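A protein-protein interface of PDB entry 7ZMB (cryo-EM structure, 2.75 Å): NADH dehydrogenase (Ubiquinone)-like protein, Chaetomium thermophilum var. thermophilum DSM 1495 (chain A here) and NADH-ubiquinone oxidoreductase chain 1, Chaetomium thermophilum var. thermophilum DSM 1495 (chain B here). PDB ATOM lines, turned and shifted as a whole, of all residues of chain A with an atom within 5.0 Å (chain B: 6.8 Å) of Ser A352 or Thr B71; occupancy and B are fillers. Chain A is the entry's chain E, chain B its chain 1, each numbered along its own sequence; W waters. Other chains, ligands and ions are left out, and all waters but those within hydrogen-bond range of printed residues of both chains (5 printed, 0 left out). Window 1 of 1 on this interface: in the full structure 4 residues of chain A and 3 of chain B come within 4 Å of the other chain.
Water W5 lies within hydrogen-bond range of the backbone carbonyl oxygen (O) of Gln B72, the side-chain hydroxyl (OG) of Ser A352, the side-chain amide nitrogen (ND2) of Asn B133 and the side-chain amide oxygen (OD1) of Asn B74.
Water W4 lies within hydrogen-bond range of O of Thr B71, N of Ser A352 and O of Ala B73.
Water W1 lies within hydrogen-bond range of the backbone carbonyl oxygen (O) of Arg A350 (2.7 Å) and the backbone carbonyl oxygen (O) of Thr B71 (2.9 Å).
Water W3 bridges the side-chain hydroxyl of Thr B71 and the side-chain hydroxyl of Tyr A355.
Water W2 lies within hydrogen-bond range of the side-chain amide nitrogen (ND2) of Asn B74 and the side-chain hydroxyl (OG) of Ser A352.
NH1 of Arg A350 lies within hydrogen-bond range of O of Tyr A355, 3.5 Å away.
The backbone carbonyl oxygen of Gln B72 lies within hydrogen-bond range of the side-chain amide nitrogen of Asn B133, at 3.0 Å.
The guanidinium group of Arg A350 lies within hydrogen-bond range of the backbone carbonyl oxygen of Tyr A354, 3.5 Å away.
The side-chain hydroxyl (OG1) of Thr B71 is in hydrogen-bond range of the side-chain amide oxygen (OE1) of Gln B72 (3.3 Å).
Thr B71 touches Pro A348 (CG2 to O, 3.0 Å).
Thr B71 touches Arg A350 (O to O, 3.8 Å).
N of Ser A352 touches O of Thr B71 (3.9 Å).
O of Gln B72 touches CB of Ser A352 (3.5 Å).
Ser A352 touches Asn B133 (CB to ND2, 3.9 Å).
OG1 of Thr B71 touches CE2 of Tyr A355 (3.9 Å).
Tyr A355 touches Gln B72 (CG to OE1, 3.3 Å).
Printed residues of chain B within 4 Å of Arg A350: Thr B71.
Of chain B, only Thr B71, Gln B72 and Asn B133 come within 4 Å of Ser A352.
Of the printed residues of chain B, Tyr A355 touches Thr B71 (3.9 Å) and Gln B72 (3.3 Å).
Of chain A, only Pro A348 (3.0 Å), Arg A350 (3.8 Å), Ser A352 (3.9 Å) and Tyr A355 (3.9 Å) come within 4 Å of Thr B71.
Ala B132 touches none of the printed residues of chain A.
Of the 10 printed residues of chain B, 3 touch a printed residue of chain A.
Among the printed residues, 7 pairs touch across the chains.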
ATOM      1  N   PRO A 348     -30.295   8.158   2.532  1.00  0.00           N
ATOM      2  CA  PRO A 348     -30.492   9.179   3.573  1.00  0.00           C
ATOM      3  C   PRO A 348     -30.196   8.708   4.987  1.00  0.00           C
ATOM      4  O   PRO A 348     -30.070   9.526   5.896  1.00  0.00           O
ATOM      5  CB  PRO A 348     -31.976   9.529   3.433  1.00  0.00           C
ATOM      6  CG  PRO A 348     -32.289   9.257   2.051  1.00  0.00           C
ATOM      7  CD  PRO A 348     -31.400   8.170   1.560  1.00  0.00           C
ATOM      8  N   ARG A 350     -27.634   6.538   5.814  1.00  0.00           N
ATOM      9  CA  ARG A 350     -26.225   6.134   6.034  1.00  0.00           C
ATOM     10  C   ARG A 350     -25.566   7.171   6.936  1.00  0.00           C
ATOM     11  O   ARG A 350     -25.839   8.365   6.746  1.00  0.00           O
ATOM     12  CB  ARG A 350     -25.442   6.049   4.720  1.00  0.00           C
ATOM     13  CG  ARG A 350     -25.720   4.811   3.886  1.00  0.00           C
ATOM     14  CD  ARG A 350     -24.794   4.842   2.692  1.00  0.00           C
ATOM     15  NE  ARG A 350     -24.517   3.530   2.136  1.00  0.00           N
ATOM     16  CZ  ARG A 350     -23.781   3.328   1.054  1.00  0.00           C
ATOM     17  NH1 ARG A 350     -23.263   4.359   0.414  1.00  0.00           N
ATOM     18  NH2 ARG A 350     -23.574   2.102   0.611  1.00  0.00           N
ATOM     19  N   PRO A 351     -24.696   6.778   7.889  1.00  0.00           N
ATOM     20  CA  PRO A 351     -23.970   7.740   8.700  1.00  0.00           C
ATOM     21  C   PRO A 351     -22.977   8.468   7.790  1.00  0.00           C
ATOM     22  O   PRO A 351     -22.583   7.910   6.792  1.00  0.00           O
ATOM     23  CB  PRO A 351     -23.260   6.890   9.757  1.00  0.00           C
ATOM     24  CG  PRO A 351     -23.109   5.542   9.104  1.00  0.00           C
ATOM     25  CD  PRO A 351     -24.314   5.405   8.199  1.00  0.00           C
ATOM     26  N   SER A 352     -22.623   9.695   8.143  1.00  0.00           N
ATOM     27  CA  SER A 352     -21.681  10.519   7.346  1.00  0.00           C
ATOM     28  C   SER A 352     -20.419   9.751   6.931  1.00  0.00           C
ATOM     29  O   SER A 352     -19.969   9.966   5.803  1.00  0.00           O
ATOM     30  CB  SER A 352     -21.334  11.731   8.138  1.00  0.00           C
ATOM     31  OG  SER A 352     -20.708  11.365   9.355  1.00  0.00           O
ATOM     32  N   THR A 353     -19.846   8.929   7.815  1.00  0.00           N
ATOM     33  CA  THR A 353     -18.579   8.210   7.531  1.00  0.00           C
ATOM     34  C   THR A 353     -18.757   7.296   6.326  1.00  0.00           C
ATOM     35  O   THR A 353     -17.819   7.188   5.520  1.00  0.00           O
ATOM     36  CB  THR A 353     -18.143   7.380   8.745  1.00  0.00           C
ATOM     37  OG1 THR A 353     -18.257   8.205   9.905  1.00  0.00           O
ATOM     38  CG2 THR A 353     -16.734   6.847   8.631  1.00  0.00           C
ATOM     39  N   TYR A 354     -19.911   6.649   6.214  1.00  0.00           N
ATOM     40  CA  TYR A 354     -20.092   5.657   5.124  1.00  0.00           C
ATOM     41  C   TYR A 354     -20.971   6.210   4.009  1.00  0.00           C
ATOM     42  O   TYR A 354     -21.287   5.455   3.086  1.00  0.00           O
ATOM     43  CB  TYR A 354     -20.597   4.341   5.717  1.00  0.00           C
ATOM     44  CG  TYR A 354     -19.772   3.853   6.877  1.00  0.00           C
ATOM     45  CD1 TYR A 354     -18.558   3.223   6.670  1.00  0.00           C
ATOM     46  CD2 TYR A 354     -20.194   4.035   8.183  1.00  0.00           C
ATOM     47  CE1 TYR A 354     -17.789   2.776   7.731  1.00  0.00           C
ATOM     48  CE2 TYR A 354     -19.438   3.597   9.256  1.00  0.00           C
ATOM     49  CZ  TYR A 354     -18.230   2.963   9.028  1.00  0.00           C
ATOM     50  OH  TYR A 354     -17.477   2.526  10.079  1.00  0.00           O
ATOM     51  N   TYR A 355     -21.383   7.473   4.103  1.00  0.00           N
ATOM     52  CA  TYR A 355     -22.338   8.026   3.108  1.00  0.00           C
ATOM     53  C   TYR A 355     -21.733   8.084   1.698  1.00  0.00           C
ATOM     54  O   TYR A 355     -22.441   7.698   0.755  1.00  0.00           O
ATOM     55  CB  TYR A 355     -22.818   9.399   3.582  1.00  0.00           C
ATOM     56  CG  TYR A 355     -23.925  10.010   2.758  1.00  0.00           C
ATOM     57  CD1 TYR A 355     -23.650  10.721   1.602  1.00  0.00           C
ATOM     58  CD2 TYR A 355     -25.249   9.884   3.142  1.00  0.00           C
ATOM     59  CE1 TYR A 355     -24.662  11.274   0.837  1.00  0.00           C
ATOM     60  CE2 TYR A 355     -26.272  10.441   2.396  1.00  0.00           C
ATOM     61  CZ  TYR A 355     -25.978  11.136   1.238  1.00  0.00           C
ATOM     62  OH  TYR A 355     -26.983  11.684   0.496  1.00  0.00           O
ATOM     63  N   ASP A 356     -20.480   8.520   1.554  1.00  0.00           N
ATOM     64  CA  ASP A 356     -19.860   8.737   0.217  1.00  0.00           C
ATOM     65  C   ASP A 356     -19.533   7.426  -0.489  1.00  0.00           C
ATOM     66  O   ASP A 356     -19.019   7.484  -1.606  1.00  0.00           O
ATOM     67  CB  ASP A 356     -18.571   9.548   0.332  1.00  0.00           C
ATOM     68  CG  ASP A 356     -18.335  10.470  -0.853  1.00  0.00           C
ATOM     69  OD1 ASP A 356     -19.238  10.566  -1.710  1.00  0.00           O
ATOM     70  OD2 ASP A 356     -17.250  11.084  -0.910  1.00  0.00           O
ATOM     71  N   VAL B  68     -35.487  18.738  12.367  1.00  0.00           N
ATOM     72  CA  VAL B  68     -34.802  17.928  11.338  1.00  0.00           C
ATOM     73  C   VAL B  68     -33.434  17.477  11.844  1.00  0.00           C
ATOM     74  O   VAL B  68     -32.737  18.299  12.415  1.00  0.00           O
ATOM     75  CB  VAL B  68     -34.698  18.701  10.016  1.00  0.00           C
ATOM     76  CG1 VAL B  68     -33.645  18.132   9.078  1.00  0.00           C
ATOM     77  CG2 VAL B  68     -36.044  18.817   9.328  1.00  0.00           C
ATOM     78  N   GLY B  69     -33.130  16.204  11.721  1.00  0.00           N
ATOM     79  CA  GLY B  69     -31.815  15.691  11.994  1.00  0.00           C
ATOM     80  C   GLY B  69     -31.091  15.369  10.709  1.00  0.00           C
ATOM     81  O   GLY B  69     -31.375  14.370  10.043  1.00  0.00           O
ATOM     82  N   PRO B  70     -30.134  16.241  10.291  1.00  0.00           N
ATOM     83  CA  PRO B  70     -29.421  16.035   9.029  1.00  0.00           C
ATOM     84  C   PRO B  70     -28.672  14.692   8.968  1.00  0.00           C
ATOM     85  O   PRO B  70     -28.149  14.262   9.978  1.00  0.00           O
ATOM     86  CB  PRO B  70     -28.495  17.257   8.924  1.00  0.00           C
ATOM     87  CG  PRO B  70     -29.139  18.291   9.792  1.00  0.00           C
ATOM     88  CD  PRO B  70     -29.632  17.467  10.957  1.00  0.00           C
ATOM     89  N   THR B  71     -28.613  14.067   7.796  1.00  0.00           N
ATOM     90  CA  THR B  71     -27.972  12.733   7.631  1.00  0.00           C
ATOM     91  C   THR B  71     -26.464  12.828   7.834  1.00  0.00           C
ATOM     92  O   THR B  71     -25.868  11.847   8.294  1.00  0.00           O
ATOM     93  CB  THR B  71     -28.224  12.195   6.221  1.00  0.00           C
ATOM     94  OG1 THR B  71     -27.291  12.780   5.314  1.00  0.00           O
ATOM     95  CG2 THR B  71     -29.631  12.465   5.756  1.00  0.00           C
ATOM     96  N   GLN B  72     -25.877  13.961   7.472  1.00  0.00           N
ATOM     97  CA  GLN B  72     -24.415  14.143   7.602  1.00  0.00           C
ATOM     98  C   GLN B  72     -24.068  14.569   9.028  1.00  0.00           C
ATOM     99  O   GLN B  72     -22.886  14.587   9.328  1.00  0.00           O
ATOM    100  CB  GLN B  72     -23.932  15.162   6.568  1.00  0.00           C
ATOM    101  CG  GLN B  72     -24.180  14.729   5.132  1.00  0.00           C
ATOM    102  CD  GLN B  72     -23.500  13.428   4.783  1.00  0.00           C
ATOM    103  OE1 GLN B  72     -23.988  12.343   5.084  1.00  0.00           O
ATOM    104  NE2 GLN B  72     -22.359  13.529   4.123  1.00  0.00           N
ATOM    105  N   ALA B  73     -25.056  14.889   9.860  1.00  0.00           N
ATOM    106  CA  ALA B  73     -24.800  15.416  11.222  1.00  0.00           C
ATOM    107  C   ALA B  73     -24.555  14.345  12.286  1.00  0.00           C
ATOM    108  O   ALA B  73     -25.258  13.322  12.256  1.00  0.00           O
ATOM    109  CB  ALA B  73     -25.956  16.287  11.639  1.00  0.00           C
ATOM    110  N   ASN B  74     -23.598  14.580  13.191  1.00  0.00           N
ATOM    111  CA  ASN B  74     -23.410  13.698  14.369  1.00  0.00           C
ATOM    112  C   ASN B  74     -24.592  14.047  15.276  1.00  0.00           C
ATOM    113  O   ASN B  74     -24.460  15.034  16.005  1.00  0.00           O
ATOM    114  CB  ASN B  74     -22.067  13.999  15.025  1.00  0.00           C
ATOM    115  CG  ASN B  74     -20.943  13.280  14.323  1.00  0.00           C
ATOM    116  OD1 ASN B  74     -19.886  13.848  14.074  1.00  0.00           O
ATOM    117  ND2 ASN B  74     -21.184  12.031  13.970  1.00  0.00           N
ATOM    118  N   LEU B  75     -25.689  13.287  15.236  1.00  0.00           N
ATOM    119  CA  LEU B  75     -26.962  13.654  15.920  1.00  0.00           C
ATOM    120  C   LEU B  75     -26.953  13.730  17.453  1.00  0.00           C
ATOM    121  O   LEU B  75     -27.612  14.640  17.976  1.00  0.00           O
ATOM    122  CB  LEU B  75     -28.087  12.764  15.388  1.00  0.00           C
ATOM    123  CG  LEU B  75     -29.317  13.510  14.875  1.00  0.00           C
ATOM    124  CD1 LEU B  75     -28.932  14.549  13.835  1.00  0.00           C
ATOM    125  CD2 LEU B  75     -30.341  12.543  14.305  1.00  0.00           C
ATOM    126  N   ALA B 132     -23.154  19.732  12.920  1.00  0.00           N
ATOM    127  CA  ALA B 132     -24.073  19.830  11.793  1.00  0.00           C
ATOM    128  C   ALA B 132     -23.470  19.266  10.517  1.00  0.00           C
ATOM    129  O   ALA B 132     -24.197  18.735   9.673  1.00  0.00           O
ATOM    130  CB  ALA B 132     -24.475  21.284  11.584  1.00  0.00           C
ATOM    131  N   ASN B 133     -22.155  19.370  10.359  1.00  0.00           N
ATOM    132  CA  ASN B 133     -21.462  18.864   9.181  1.00  0.00           C
ATOM    133  C   ASN B 133     -21.991  19.526   7.908  1.00  0.00           C
ATOM    134  O   ASN B 133     -22.186  18.880   6.879  1.00  0.00           O
ATOM    135  CB  ASN B 133     -21.557  17.339   9.109  1.00  0.00           C
ATOM    136  CG  ASN B 133     -20.514  16.734   8.214  1.00  0.00           C
ATOM    137  OD1 ASN B 133     -20.017  17.377   7.299  1.00  0.00           O
ATOM    138  ND2 ASN B 133     -20.180  15.483   8.467  1.00  0.00           N
HETATM  139  O   HOH W   1     -27.334   9.370   8.695  1.00  0.00           O
HETATM  140  O   HOH W   2     -22.182  10.656  11.742  1.00  0.00           O
HETATM  141  O   HOH W   3     -26.675  14.039   3.000  1.00  0.00           O
HETATM  142  O   HOH W   4     -24.569  10.802  10.293  1.00  0.00           O
HETATM  143  O   HOH W   5     -21.129  13.779  10.889  1.00  0.00           O
